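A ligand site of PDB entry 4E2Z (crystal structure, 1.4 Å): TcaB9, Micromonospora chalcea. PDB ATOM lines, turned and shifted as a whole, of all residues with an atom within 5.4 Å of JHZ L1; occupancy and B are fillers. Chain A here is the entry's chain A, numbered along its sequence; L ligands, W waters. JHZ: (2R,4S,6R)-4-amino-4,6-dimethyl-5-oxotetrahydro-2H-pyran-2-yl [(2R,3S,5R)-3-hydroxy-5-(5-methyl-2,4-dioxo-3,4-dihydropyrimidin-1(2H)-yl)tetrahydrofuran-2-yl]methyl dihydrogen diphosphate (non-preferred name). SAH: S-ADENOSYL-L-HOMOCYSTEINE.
Water W2 bridges O4 of JHZ L1 (2.7 Å) and OD1 of Asn 179 (2.8 Å). Water W7 lies within hydrogen-bond range of OH of Tyr 325 (2.7 Å), N31 of JHZ L1 (2.8 Å) and NZ of Lys 395 (3.4 Å). Water W5 lies within hydrogen-bond range of the side-chain amino group of Lys 355 (2.7 Å), the side-chain carboxylate of Asp 35 (2.8 Å) and an oxygen (O4P) of JHZ L1 (2.8 Å). Water W1 lies within hydrogen-bond range of O4 of JHZ L1, O of Glu 226, OH of Tyr 224 and SG of Cys 182. Water W3 lies within hydrogen-bond range of OH of Tyr 224 (2.6 Å) and O1 of JHZ L1 (3.1 Å). Water W4 lies within hydrogen-bond range of O of Gly 84 (2.7 Å) and OG1 of Thr 351 (2.7 Å).
The backbone NH (N) of Ala 327 is in hydrogen-bond range of the side-chain carboxylate (OD1) of Asp 350 (2.8 Å). OH of Tyr 78 is in hydrogen-bond range of OE1 of Glu 226 (2.8 Å). The side-chain carboxylate (OD2) of Asp 35 lies close to the side-chain carboxylate (OE2) of Glu 226 (2.5 Å). The side-chain amino group (NZ) of Lys 330 lies within hydrogen-bond range of the side-chain amide oxygen (OD1) of Asn 387. The side-chain amide nitrogen (ND2) of Asn 387 lies close to a ring nitrogen (NE2) of His 388 (3.4 Å). The side-chain carboxylate of Glu 391 sits at hydrogen-bond distance from the side-chain hydroxyl of Ser 85, 2.9 Å away. O of Tyr 349 lies within hydrogen-bond range of N of Gly 326 (2.8 Å). N of Ala 385 lies within hydrogen-bond range of O of Tyr 325 (3.1 Å).
Asp 35 touches JHZ L1. Tyr 78 touches JHZ L1 (OH to C3M, 3.3 Å). CB of Asn 179 touches C6 of JHZ L1, 3.7 Å away. NE2 of His 256 touches C6 of JHZ L1, at 3.6 Å. Tyr 325 touches JHZ L1. CA of Gly 326 touches O4X of JHZ L1, at 3.7 Å. Ala 327 touches JHZ L1. Thr 328 touches JHZ L1. Ala 385 touches JHZ L1. OE1 of Glu 391 touches C5A of JHZ L1, 3.7 Å away. Ile 392 touches JHZ L1 (CG1 to O41, 3.4 Å). Hydrophobic or aromatic side chains within 4 Å of JHZ L1: Tyr 80, Tyr 224, His 256, Tyr 325, Ala 329, Ala 385, His 388 and Ile 392. 23 residues have an atom within 4 Å of JHZ L1: Asp 35, Tyr 78, Tyr 80, Asn 179, Tyr 224, Glu 226, His 256, Tyr 325, Gly 326, Ala 327, Thr 328, Ala 329, Lys 330, Asp 350, Thr 351, Thr 352, Lys 355, Ala 385, Asn 387, His 388, Glu 391, Ile 392 and Lys 395. The nearest printed residue that does not touch JHZ L1 is Ser 85 (4.04 Å).
OD1 of Asp 350 is in hydrogen-bond range of O3X of JHZ L1 (2.6 Å). A nitrogen (N3) of JHZ L1 lies within salt-bridge range of the side-chain carboxylate of Glu 226. OH of Tyr 80 is in hydrogen-bond range of O1P of JHZ L1. NZ of Lys 395 lies within hydrogen-bond range of O41 of JHZ L1 (2.8 Å). The backbone NH (N) of Ala 329 sits at hydrogen-bond distance from an oxygen (O4P) of JHZ L1 (2.8 Å). NZ of Lys 330 is in salt-bridge range of O3P of JHZ L1. A ring nitrogen (NE2) of His 388 sits at hydrogen-bond distance from an oxygen (O1P) of JHZ L1 (2.8 Å). The side-chain amide nitrogen (ND2) of Asn 387 lies within hydrogen-bond range of an oxygen (O2P) of JHZ L1 (2.9 Å). The side-chain amino group (NZ) of Lys 355 is in hydrogen-bond range of an oxygen (O3X) of JHZ L1. O21 of JHZ L1 sits at hydrogen-bond distance from N of Thr 351, at 3.0 Å. The side-chain hydroxyl of Thr 351 lies close to an oxygen (O21) of JHZ L1, 3.3 Å away. The side-chain hydroxyl of Tyr 224 is in hydrogen-bond range of a nitrogen (N3) of JHZ L1. The side-chain hydroxyl of Thr 352 lies within hydrogen-bond range of an oxygen (O3X) of JHZ L1 (3.3 Å). An oxygen (O) of SAH L2 lies within hydrogen-bond range of the side-chain amide nitrogen (ND2) of Asn 179 (2.9 Å). NE2 of His 183 is in hydrogen-bond range of O4' of SAH L2 (3.3 Å).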
ATOM      1  N   ASP A  35     -19.397  -9.180   4.412  1.00  0.00           N
ATOM      2  CA  ASP A  35     -20.256  -9.998   3.559  1.00  0.00           C
ATOM      3  C   ASP A  35     -21.224 -10.838   4.381  1.00  0.00           C
ATOM      4  O   ASP A  35     -21.811 -11.809   3.869  1.00  0.00           O
ATOM      5  CB  ASP A  35     -19.416 -10.824   2.556  1.00  0.00           C
ATOM      6  CG  ASP A  35     -19.208 -10.114   1.213  1.00  0.00           C
ATOM      7  OD1 ASP A  35     -20.246  -9.631   0.713  1.00  0.00           O
ATOM      8  OD2 ASP A  35     -18.081 -10.069   0.676  1.00  0.00           O
ATOM      9  N   TYR A  78     -21.060 -17.806   1.671  1.00  0.00           N
ATOM     10  CA  TYR A  78     -20.538 -16.576   1.097  1.00  0.00           C
ATOM     11  C   TYR A  78     -21.441 -16.081  -0.045  1.00  0.00           C
ATOM     12  O   TYR A  78     -21.773 -16.827  -0.958  1.00  0.00           O
ATOM     13  CB  TYR A  78     -19.149 -16.843   0.545  1.00  0.00           C
ATOM     14  CG  TYR A  78     -18.412 -15.624   0.022  1.00  0.00           C
ATOM     15  CD1 TYR A  78     -18.198 -15.501  -1.344  1.00  0.00           C
ATOM     16  CD2 TYR A  78     -17.945 -14.647   0.906  1.00  0.00           C
ATOM     17  CE1 TYR A  78     -17.479 -14.391  -1.812  1.00  0.00           C
ATOM     18  CE2 TYR A  78     -17.259 -13.522   0.428  1.00  0.00           C
ATOM     19  CZ  TYR A  78     -17.058 -13.434  -0.935  1.00  0.00           C
ATOM     20  OH  TYR A  78     -16.350 -12.362  -1.423  1.00  0.00           O
ATOM     21  N   TYR A  80     -21.260 -13.453  -2.533  1.00  0.00           N
ATOM     22  CA  TYR A  80     -20.951 -12.627  -3.727  1.00  0.00           C
ATOM     23  C   TYR A  80     -21.041 -13.526  -4.959  1.00  0.00           C
ATOM     24  O   TYR A  80     -20.382 -14.560  -5.044  1.00  0.00           O
ATOM     25  CB  TYR A  80     -19.558 -12.013  -3.674  1.00  0.00           C
ATOM     26  CG  TYR A  80     -19.278 -11.129  -4.884  1.00  0.00           C
ATOM     27  CD1 TYR A  80     -19.975  -9.933  -5.096  1.00  0.00           C
ATOM     28  CD2 TYR A  80     -18.253 -11.467  -5.780  1.00  0.00           C
ATOM     29  CE1 TYR A  80     -19.704  -9.077  -6.182  1.00  0.00           C
ATOM     30  CE2 TYR A  80     -18.001 -10.664  -6.874  1.00  0.00           C
ATOM     31  CZ  TYR A  80     -18.721  -9.493  -7.048  1.00  0.00           C
ATOM     32  OH  TYR A  80     -18.430  -8.647  -8.097  1.00  0.00           O
ATOM     33  N   GLY A  84     -23.135 -11.589 -11.631  1.00  0.00           N
ATOM     34  CA  GLY A  84     -24.157 -10.530 -11.575  1.00  0.00           C
ATOM     35  C   GLY A  84     -23.926  -9.269 -12.401  1.00  0.00           C
ATOM     36  O   GLY A  84     -24.843  -8.469 -12.554  1.00  0.00           O
ATOM     37  N   SER A  85     -22.761  -9.056 -13.015  1.00  0.00           N
ATOM     38  CA  SER A  85     -22.451  -7.820 -13.740  1.00  0.00           C
ATOM     39  C   SER A  85     -22.148  -8.301 -15.163  1.00  0.00           C
ATOM     40  O   SER A  85     -21.277  -9.157 -15.386  1.00  0.00           O
ATOM     41  CB  SER A  85     -21.137  -7.243 -13.201  1.00  0.00           C
ATOM     42  OG  SER A  85     -20.592  -6.291 -14.115  1.00  0.00           O
ATOM     43  N   ASN A 179      -9.287 -10.428  -7.979  1.00  0.00           N
ATOM     44  CA  ASN A 179     -10.005 -10.022  -6.752  1.00  0.00           C
ATOM     45  C   ASN A 179      -9.945 -11.047  -5.614  1.00  0.00           C
ATOM     46  O   ASN A 179     -10.890 -11.131  -4.843  1.00  0.00           O
ATOM     47  CB  ASN A 179     -11.444  -9.598  -7.096  1.00  0.00           C
ATOM     48  CG  ASN A 179     -11.440  -8.585  -8.224  1.00  0.00           C
ATOM     49  OD1 ASN A 179     -10.841  -7.525  -8.055  1.00  0.00           O
ATOM     50  ND2 ASN A 179     -12.048  -8.934  -9.376  1.00  0.00           N
ATOM     51  N   CYS A 182      -5.475 -10.192  -3.215  1.00  0.00           N
ATOM     52  CA  CYS A 182      -5.747  -9.032  -2.312  1.00  0.00           C
ATOM     53  C   CYS A 182      -6.224  -9.534  -0.931  1.00  0.00           C
ATOM     54  O   CYS A 182      -5.958  -8.809   0.047  1.00  0.00           O
ATOM     55  CB  CYS A 182      -6.653  -7.881  -2.921  1.00  0.00           C
ATOM     56  SG  CYS A 182      -8.297  -8.411  -3.074  1.00  0.00           S
ATOM     57  N   HIS A 183      -6.946 -10.651  -0.825  1.00  0.00           N
ATOM     58  CA  HIS A 183      -7.479 -10.974   0.507  1.00  0.00           C
ATOM     59  C   HIS A 183      -6.805 -12.150   1.196  1.00  0.00           C
ATOM     60  O   HIS A 183      -7.365 -12.664   2.162  1.00  0.00           O
ATOM     61  CB  HIS A 183      -8.996 -10.949   0.626  1.00  0.00           C
ATOM     62  CG  HIS A 183      -9.711 -11.866  -0.304  1.00  0.00           C
ATOM     63  ND1 HIS A 183     -10.660 -11.415  -1.196  1.00  0.00           N
ATOM     64  CD2 HIS A 183      -9.696 -13.221  -0.408  1.00  0.00           C
ATOM     65  CE1 HIS A 183     -11.169 -12.464  -1.837  1.00  0.00           C
ATOM     66  NE2 HIS A 183     -10.589 -13.565  -1.391  1.00  0.00           N
ATOM     67  N   TYR A 224     -11.570  -2.931   3.535  1.00  0.00           N
ATOM     68  CA  TYR A 224     -12.524  -3.689   4.372  1.00  0.00           C
ATOM     69  C   TYR A 224     -11.913  -5.072   4.618  1.00  0.00           C
ATOM     70  O   TYR A 224     -10.799  -5.323   4.159  1.00  0.00           O
ATOM     71  CB  TYR A 224     -13.929  -3.728   3.733  1.00  0.00           C
ATOM     72  CG  TYR A 224     -14.012  -4.406   2.362  1.00  0.00           C
ATOM     73  CD1 TYR A 224     -14.413  -5.749   2.232  1.00  0.00           C
ATOM     74  CD2 TYR A 224     -13.653  -3.715   1.214  1.00  0.00           C
ATOM     75  CE1 TYR A 224     -14.508  -6.349   0.965  1.00  0.00           C
ATOM     76  CE2 TYR A 224     -13.740  -4.290  -0.034  1.00  0.00           C
ATOM     77  CZ  TYR A 224     -14.103  -5.621  -0.149  1.00  0.00           C
ATOM     78  OH  TYR A 224     -14.120  -6.160  -1.424  1.00  0.00           O
ATOM     79  N   GLU A 226     -12.155  -8.139   3.503  1.00  0.00           N
ATOM     80  CA  GLU A 226     -11.645  -8.834   2.297  1.00  0.00           C
ATOM     81  C   GLU A 226     -10.805  -7.956   1.345  1.00  0.00           C
ATOM     82  O   GLU A 226     -10.764  -8.071   0.092  1.00  0.00           O
ATOM     83  CB  GLU A 226     -12.787  -9.415   1.454  1.00  0.00           C
ATOM     84  CG  GLU A 226     -13.735 -10.291   2.256  1.00  0.00           C
ATOM     85  CD  GLU A 226     -15.028 -10.552   1.483  1.00  0.00           C
ATOM     86  OE1 GLU A 226     -14.939 -10.587   0.219  1.00  0.00           O
ATOM     87  OE2 GLU A 226     -16.114 -10.730   2.105  1.00  0.00           O
ATOM     88  N   HIS A 256     -13.798  -2.394 -11.150  1.00  0.00           N
ATOM     89  CA  HIS A 256     -13.655  -2.319  -9.686  1.00  0.00           C
ATOM     90  C   HIS A 256     -13.006  -1.064  -9.148  1.00  0.00           C
ATOM     91  O   HIS A 256     -12.307  -1.155  -8.114  1.00  0.00           O
ATOM     92  CB  HIS A 256     -13.102  -3.622  -9.106  1.00  0.00           C
ATOM     93  CG  HIS A 256     -14.047  -4.775  -9.232  1.00  0.00           C
ATOM     94  ND1 HIS A 256     -15.288  -4.790  -8.635  1.00  0.00           N
ATOM     95  CD2 HIS A 256     -13.934  -5.945  -9.928  1.00  0.00           C
ATOM     96  CE1 HIS A 256     -15.916  -5.908  -8.982  1.00  0.00           C
ATOM     97  NE2 HIS A 256     -15.105  -6.635  -9.737  1.00  0.00           N
ATOM     98  N   TYR A 325     -27.894   2.193  -3.402  1.00  0.00           N
ATOM     99  CA  TYR A 325     -28.006   1.239  -4.512  1.00  0.00           C
ATOM    100  C   TYR A 325     -26.698   0.435  -4.595  1.00  0.00           C
ATOM    101  O   TYR A 325     -25.576   0.941  -4.770  1.00  0.00           O
ATOM    102  CB  TYR A 325     -28.224   2.044  -5.808  1.00  0.00           C
ATOM    103  CG  TYR A 325     -28.760   1.182  -6.932  1.00  0.00           C
ATOM    104  CD1 TYR A 325     -28.061   0.083  -7.418  1.00  0.00           C
ATOM    105  CD2 TYR A 325     -30.004   1.501  -7.495  1.00  0.00           C
ATOM    106  CE1 TYR A 325     -28.625  -0.703  -8.457  1.00  0.00           C
ATOM    107  CE2 TYR A 325     -30.556   0.720  -8.529  1.00  0.00           C
ATOM    108  CZ  TYR A 325     -29.867  -0.369  -9.018  1.00  0.00           C
ATOM    109  OH  TYR A 325     -30.435  -1.095 -10.058  1.00  0.00           O
ATOM    110  N   GLY A 326     -26.866  -0.881  -4.414  1.00  0.00           N
ATOM    111  CA  GLY A 326     -25.832  -1.901  -4.411  1.00  0.00           C
ATOM    112  C   GLY A 326     -25.424  -2.229  -2.991  1.00  0.00           C
ATOM    113  O   GLY A 326     -24.870  -1.405  -2.279  1.00  0.00           O
ATOM    114  N   ALA A 327     -25.661  -3.464  -2.548  1.00  0.00           N
ATOM    115  CA  ALA A 327     -25.264  -3.903  -1.189  1.00  0.00           C
ATOM    116  C   ALA A 327     -23.853  -4.471  -1.230  1.00  0.00           C
ATOM    117  O   ALA A 327     -23.621  -5.679  -1.022  1.00  0.00           O
ATOM    118  CB  ALA A 327     -26.254  -4.961  -0.628  1.00  0.00           C
ATOM    119  N   THR A 328     -22.935  -3.586  -1.646  1.00  0.00           N
ATOM    120  CA  THR A 328     -21.538  -3.991  -1.766  1.00  0.00           C
ATOM    121  C   THR A 328     -20.890  -4.407  -0.454  1.00  0.00           C
ATOM    122  O   THR A 328     -21.289  -3.886   0.599  1.00  0.00           O
ATOM    123  CB  THR A 328     -20.738  -2.793  -2.348  1.00  0.00           C
ATOM    124  OG1 THR A 328     -20.868  -1.689  -1.438  1.00  0.00           O
ATOM    125  CG2 THR A 328     -21.229  -2.355  -3.773  1.00  0.00           C
ATOM    126  N   ALA A 329     -19.921  -5.320  -0.499  1.00  0.00           N
ATOM    127  CA  ALA A 329     -19.027  -5.449   0.639  1.00  0.00           C
ATOM    128  C   ALA A 329     -18.387  -4.132   1.088  1.00  0.00           C
ATOM    129  O   ALA A 329     -18.297  -3.793   2.267  1.00  0.00           O
ATOM    130  CB  ALA A 329     -17.978  -6.516   0.327  1.00  0.00           C
ATOM    131  N   LYS A 330     -17.962  -3.323   0.114  1.00  0.00           N
ATOM    132  CA  LYS A 330     -17.314  -2.036   0.352  1.00  0.00           C
ATOM    133  C   LYS A 330     -18.172  -1.118   1.223  1.00  0.00           C
ATOM    134  O   LYS A 330     -17.641  -0.323   2.041  1.00  0.00           O
ATOM    135  CB  LYS A 330     -17.133  -1.318  -1.012  1.00  0.00           C
ATOM    136  CG  LYS A 330     -16.020  -1.992  -1.867  1.00  0.00           C
ATOM    137  CD  LYS A 330     -15.704  -1.161  -3.144  1.00  0.00           C
ATOM    138  CE  LYS A 330     -16.873  -0.916  -4.128  1.00  0.00           C
ATOM    139  NZ  LYS A 330     -17.292  -2.173  -4.842  1.00  0.00           N
ATOM    140  N   TYR A 349     -30.891  -1.232  -2.452  1.00  0.00           N
ATOM    141  CA  TYR A 349     -31.392  -2.134  -3.512  1.00  0.00           C
ATOM    142  C   TYR A 349     -30.262  -2.999  -4.093  1.00  0.00           C
ATOM    143  O   TYR A 349     -29.139  -2.510  -4.295  1.00  0.00           O
ATOM    144  CB  TYR A 349     -32.114  -1.289  -4.579  1.00  0.00           C
ATOM    145  CG  TYR A 349     -33.317  -0.616  -3.954  1.00  0.00           C
ATOM    146  CD1 TYR A 349     -34.492  -1.359  -3.789  1.00  0.00           C
ATOM    147  CD2 TYR A 349     -33.240   0.672  -3.411  1.00  0.00           C
ATOM    148  CE1 TYR A 349     -35.580  -0.802  -3.155  1.00  0.00           C
ATOM    149  CE2 TYR A 349     -34.313   1.247  -2.769  1.00  0.00           C
ATOM    150  CZ  TYR A 349     -35.470   0.493  -2.679  1.00  0.00           C
ATOM    151  OH  TYR A 349     -36.512   1.087  -2.012  1.00  0.00           O
ATOM    152  N   ASP A 350     -30.507  -4.286  -4.321  1.00  0.00           N
ATOM    153  CA  ASP A 350     -29.479  -5.211  -4.797  1.00  0.00           C
ATOM    154  C   ASP A 350     -29.994  -6.426  -5.602  1.00  0.00           C
ATOM    155  O   ASP A 350     -31.068  -6.924  -5.236  1.00  0.00           O
ATOM    156  CB  ASP A 350     -28.691  -5.723  -3.575  1.00  0.00           C
ATOM    157  CG  ASP A 350     -27.395  -6.391  -3.998  1.00  0.00           C
ATOM    158  OD1 ASP A 350     -26.352  -5.704  -4.088  1.00  0.00           O
ATOM    159  OD2 ASP A 350     -27.435  -7.618  -4.230  1.00  0.00           O
ATOM    160  N   THR A 351     -29.312  -6.857  -6.660  1.00  0.00           N
ATOM    161  CA  THR A 351     -29.764  -8.004  -7.459  1.00  0.00           C
ATOM    162  C   THR A 351     -29.448  -9.377  -6.906  1.00  0.00           C
ATOM    163  O   THR A 351     -29.834 -10.360  -7.551  1.00  0.00           O
ATOM    164  CB  THR A 351     -29.185  -7.856  -8.881  1.00  0.00           C
ATOM    165  OG1 THR A 351     -27.773  -7.696  -8.794  1.00  0.00           O
ATOM    166  CG2 THR A 351     -29.818  -6.697  -9.637  1.00  0.00           C
ATOM    167  N   THR A 352     -28.765  -9.482  -5.780  1.00  0.00           N
ATOM    168  CA  THR A 352     -28.341 -10.784  -5.277  1.00  0.00           C
ATOM    169  C   THR A 352     -29.393 -11.415  -4.362  1.00  0.00           C
ATOM    170  O   THR A 352     -29.656 -10.879  -3.282  1.00  0.00           O
ATOM    171  CB  THR A 352     -27.000 -10.680  -4.493  1.00  0.00           C
ATOM    172  OG1 THR A 352     -26.079  -9.782  -5.147  1.00  0.00           O
ATOM    173  CG2 THR A 352     -26.294 -12.001  -4.200  1.00  0.00           C
ATOM    174  N   LYS A 355     -28.701 -11.751  -0.590  1.00  0.00           N
ATOM    175  CA  LYS A 355     -28.560 -10.540   0.234  1.00  0.00           C
ATOM    176  C   LYS A 355     -29.922  -9.895   0.445  1.00  0.00           C
ATOM    177  O   LYS A 355     -30.028  -9.028   1.317  1.00  0.00           O
ATOM    178  CB  LYS A 355     -27.691  -9.466  -0.455  1.00  0.00           C
ATOM    179  CG  LYS A 355     -26.244  -9.954  -0.691  1.00  0.00           C
ATOM    180  CD  LYS A 355     -25.432  -8.860  -1.435  1.00  0.00           C
ATOM    181  CE  LYS A 355     -23.981  -9.286  -1.613  1.00  0.00           C
ATOM    182  NZ  LYS A 355     -23.117  -8.179  -2.120  1.00  0.00           N
ATOM    183  N   ALA A 370     -33.572  -5.232  -6.448  1.00  0.00           N
ATOM    184  CA  ALA A 370     -33.489  -4.054  -7.313  1.00  0.00           C
ATOM    185  C   ALA A 370     -34.743  -3.838  -8.145  1.00  0.00           C
ATOM    186  O   ALA A 370     -35.118  -2.721  -8.515  1.00  0.00           O
ATOM    187  CB  ALA A 370     -32.299  -4.208  -8.257  1.00  0.00           C
ATOM    188  N   ALA A 385     -22.567   0.984  -5.340  1.00  0.00           N
ATOM    189  CA  ALA A 385     -21.925   0.247  -6.441  1.00  0.00           C
ATOM    190  C   ALA A 385     -21.409   1.215  -7.493  1.00  0.00           C
ATOM    191  O   ALA A 385     -21.741   1.096  -8.691  1.00  0.00           O
ATOM    192  CB  ALA A 385     -22.911  -0.801  -7.027  1.00  0.00           C
ATOM    193  N   ASN A 387     -18.548   1.551  -8.812  1.00  0.00           N
ATOM    194  CA  ASN A 387     -17.672   0.905  -9.798  1.00  0.00           C
ATOM    195  C   ASN A 387     -18.482   0.325 -10.971  1.00  0.00           C
ATOM    196  O   ASN A 387     -17.901   0.029 -12.030  1.00  0.00           O
ATOM    197  CB  ASN A 387     -16.814  -0.167  -9.136  1.00  0.00           C
ATOM    198  CG  ASN A 387     -17.588  -1.101  -8.223  1.00  0.00           C
ATOM    199  OD1 ASN A 387     -18.256  -0.670  -7.260  1.00  0.00           O
ATOM    200  ND2 ASN A 387     -17.522  -2.413  -8.489  1.00  0.00           N
ATOM    201  N   HIS A 388     -19.789   0.219 -10.729  1.00  0.00           N
ATOM    202  CA  HIS A 388     -20.723  -0.263 -11.756  1.00  0.00           C
ATOM    203  C   HIS A 388     -21.658   0.839 -12.270  1.00  0.00           C
ATOM    204  O   HIS A 388     -22.721   0.509 -12.806  1.00  0.00           O
ATOM    205  CB  HIS A 388     -21.581  -1.390 -11.187  1.00  0.00           C
ATOM    206  CG  HIS A 388     -20.836  -2.634 -10.796  1.00  0.00           C
ATOM    207  ND1 HIS A 388     -20.300  -3.457 -11.760  1.00  0.00           N
ATOM    208  CD2 HIS A 388     -20.506  -3.191  -9.610  1.00  0.00           C
ATOM    209  CE1 HIS A 388     -19.753  -4.516 -11.191  1.00  0.00           C
ATOM    210  NE2 HIS A 388     -19.867  -4.377  -9.875  1.00  0.00           N
ATOM    211  N   GLU A 391     -23.156   0.499 -16.037  1.00  0.00           N
ATOM    212  CA  GLU A 391     -24.064  -0.634 -16.191  1.00  0.00           C
ATOM    213  C   GLU A 391     -25.382  -0.373 -15.435  1.00  0.00           C
ATOM    214  O   GLU A 391     -26.506  -0.602 -15.939  1.00  0.00           O
ATOM    215  CB  GLU A 391     -23.403  -1.879 -15.590  1.00  0.00           C
ATOM    216  CG  GLU A 391     -24.291  -3.109 -15.674  1.00  0.00           C
ATOM    217  CD  GLU A 391     -23.573  -4.417 -15.381  1.00  0.00           C
ATOM    218  OE1 GLU A 391     -24.251  -5.464 -15.188  1.00  0.00           O
ATOM    219  OE2 GLU A 391     -22.316  -4.408 -15.398  1.00  0.00           O
ATOM    220  N   ILE A 392     -25.290   0.110 -14.201  1.00  0.00           N
ATOM    221  CA  ILE A 392     -26.459   0.400 -13.381  1.00  0.00           C
ATOM    222  C   ILE A 392     -27.297   1.534 -13.967  1.00  0.00           C
ATOM    223  O   ILE A 392     -28.525   1.461 -14.144  1.00  0.00           O
ATOM    224  CB  ILE A 392     -26.094   0.656 -11.883  1.00  0.00           C
ATOM    225  CG1 ILE A 392     -25.719  -0.684 -11.249  1.00  0.00           C
ATOM    226  CG2 ILE A 392     -27.336   1.188 -11.123  1.00  0.00           C
ATOM    227  CD1 ILE A 392     -25.033  -0.490  -9.883  1.00  0.00           C
ATOM    228  N   LYS A 395     -29.486   0.739 -16.846  1.00  0.00           N
ATOM    229  CA  LYS A 395     -30.654  -0.061 -16.493  1.00  0.00           C
ATOM    230  C   LYS A 395     -31.664   0.823 -15.768  1.00  0.00           C
ATOM    231  O   LYS A 395     -32.813   0.412 -15.647  1.00  0.00           O
ATOM    232  CB  LYS A 395     -30.276  -1.244 -15.599  1.00  0.00           C
ATOM    233  CG  LYS A 395     -29.685  -2.393 -16.390  1.00  0.00           C
ATOM    234  CD  LYS A 395     -29.614  -3.678 -15.600  1.00  0.00           C
ATOM    235  CE  LYS A 395     -28.436  -3.550 -14.668  1.00  0.00           C
ATOM    236  NZ  LYS A 395     -28.490  -4.778 -13.831  1.00  0.00           N
HETATM  237  P   JHZ L   1     -19.340  -5.291  -6.422  1.00  0.00           P
HETATM  238  C1  JHZ L   1     -17.090  -8.146  -3.695  1.00  0.00           C
HETATM  239  O1  JHZ L   1     -16.988  -6.747  -3.426  1.00  0.00           O
HETATM  240  C2  JHZ L   1     -16.354  -8.964  -2.627  1.00  0.00           C
HETATM  241  P2  JHZ L   1     -18.277  -5.826  -3.644  1.00  0.00           P
HETATM  242  C3  JHZ L   1     -14.888  -9.141  -3.066  1.00  0.00           C
HETATM  243  N3  JHZ L   1     -14.004  -9.165  -1.894  1.00  0.00           N
HETATM  244  C4  JHZ L   1     -14.429  -8.192  -4.160  1.00  0.00           C
HETATM  245  O4  JHZ L   1     -13.333  -7.647  -4.124  1.00  0.00           O
HETATM  246  C5  JHZ L   1     -15.334  -7.839  -5.319  1.00  0.00           C
HETATM  247  O5  JHZ L   1     -16.594  -8.425  -5.012  1.00  0.00           O
HETATM  248  C6  JHZ L   1     -14.905  -8.437  -6.661  1.00  0.00           C
HETATM  249  C1X JHZ L   1     -25.196  -5.262  -6.966  1.00  0.00           C
HETATM  250  N11 JHZ L   1     -25.526  -4.895  -8.353  1.00  0.00           N
HETATM  251  O1P JHZ L   1     -19.282  -6.085  -7.730  1.00  0.00           O
HETATM  252  C2X JHZ L   1     -24.615  -6.673  -6.982  1.00  0.00           C
HETATM  253  C21 JHZ L   1     -26.803  -4.567  -8.606  1.00  0.00           C
HETATM  254  O21 JHZ L   1     -27.739  -4.523  -7.786  1.00  0.00           O
HETATM  255  O2P JHZ L   1     -19.039  -3.836  -6.494  1.00  0.00           O
HETATM  256  C3X JHZ L   1     -23.593  -6.669  -5.856  1.00  0.00           C
HETATM  257  O3X JHZ L   1     -24.204  -7.095  -4.601  1.00  0.00           O
HETATM  258  N31 JHZ L   1     -27.150  -4.188  -9.881  1.00  0.00           N
HETATM  259  C3M JHZ L   1     -14.699 -10.556  -3.651  1.00  0.00           C
HETATM  260  O3P JHZ L   1     -17.917  -4.414  -3.292  1.00  0.00           O
HETATM  261  C4X JHZ L   1     -23.134  -5.216  -5.784  1.00  0.00           C
HETATM  262  O4X JHZ L   1     -24.149  -4.464  -6.424  1.00  0.00           O
HETATM  263  C41 JHZ L   1     -26.249  -4.237 -10.888  1.00  0.00           C
HETATM  264  O41 JHZ L   1     -26.577  -3.881 -12.053  1.00  0.00           O
HETATM  265  O4P JHZ L   1     -19.506  -6.409  -3.022  1.00  0.00           O
HETATM  266  C5X JHZ L   1     -21.884  -4.881  -6.588  1.00  0.00           C
HETATM  267  O5X JHZ L   1     -20.814  -5.452  -5.840  1.00  0.00           O
HETATM  268  C51 JHZ L   1     -24.827  -4.559 -10.606  1.00  0.00           C
HETATM  269  C5A JHZ L   1     -23.761  -4.582 -11.667  1.00  0.00           C
HETATM  270  C61 JHZ L   1     -24.544  -4.898  -9.282  1.00  0.00           C
HETATM  271  OPP JHZ L   1     -18.472  -5.935  -5.230  1.00  0.00           O
HETATM  272  N   SAH L   2     -12.604 -14.148  -9.238  1.00  0.00           N
HETATM  273  CA  SAH L   2     -13.968 -13.671  -8.825  1.00  0.00           C
HETATM  274  CB  SAH L   2     -14.051 -13.921  -7.321  1.00  0.00           C
HETATM  275  CG  SAH L   2     -14.323 -12.722  -6.433  1.00  0.00           C
HETATM  276  SD  SAH L   2     -14.791 -13.418  -4.873  1.00  0.00           S
HETATM  277  C   SAH L   2     -14.126 -12.271  -9.355  1.00  0.00           C
HETATM  278  O   SAH L   2     -13.119 -11.636  -9.687  1.00  0.00           O
HETATM  279  OXT SAH L   2     -15.234 -11.771  -9.397  1.00  0.00           O
HETATM  280  C5' SAH L   2     -13.305 -13.902  -4.038  1.00  0.00           C
HETATM  281  C4' SAH L   2     -13.297 -15.435  -3.955  1.00  0.00           C
HETATM  282  O4' SAH L   2     -12.058 -15.812  -3.351  1.00  0.00           O
HETATM  283  C3' SAH L   2     -14.432 -15.972  -3.071  1.00  0.00           C
HETATM  284  O3' SAH L   2     -15.286 -16.763  -3.919  1.00  0.00           O
HETATM  285  C2' SAH L   2     -13.699 -16.835  -2.034  1.00  0.00           C
HETATM  286  O2' SAH L   2     -14.278 -18.045  -1.515  1.00  0.00           O
HETATM  287  C1' SAH L   2     -12.387 -17.098  -2.774  1.00  0.00           C
HETATM  288  N9  SAH L   2     -11.210 -17.409  -1.913  1.00  0.00           N
HETATM  289  C8  SAH L   2     -10.809 -16.909  -0.707  1.00  0.00           C
HETATM  290  N7  SAH L   2      -9.614 -17.354  -0.294  1.00  0.00           N
HETATM  291  C5  SAH L   2      -9.206 -18.254  -1.234  1.00  0.00           C
HETATM  292  C6  SAH L   2      -8.013 -19.097  -1.436  1.00  0.00           C
HETATM  293  N6  SAH L   2      -7.013 -19.174  -0.525  1.00  0.00           N
HETATM  294  N1  SAH L   2      -8.102 -19.841  -2.557  1.00  0.00           N
HETATM  295  C2  SAH L   2      -9.043 -19.813  -3.533  1.00  0.00           C
HETATM  296  N3  SAH L   2     -10.145 -19.052  -3.412  1.00  0.00           N
HETATM  297  C4  SAH L   2     -10.212 -18.240  -2.315  1.00  0.00           C
HETATM  298  O   HOH W   1     -11.091  -6.525  -2.497  1.00  0.00           O
HETATM  299  O   HOH W   2     -11.589  -6.203  -5.650  1.00  0.00           O
HETATM  300  O   HOH W   3     -14.744  -4.650  -3.445  1.00  0.00           O
HETATM  301  O   HOH W   4     -27.076  -7.439 -11.409  1.00  0.00           O
HETATM  302  O   HOH W   5     -20.477  -8.823  -1.959  1.00  0.00           O
HETATM  303  O   HOH W   6     -23.150  -9.576  -8.112  1.00  0.00           O
HETATM  304  O   HOH W   7     -29.678  -3.549 -10.892  1.00  0.00           O
HETATM  305  O   HOH W   8     -22.024  -7.369  -9.348  1.00  0.00           O
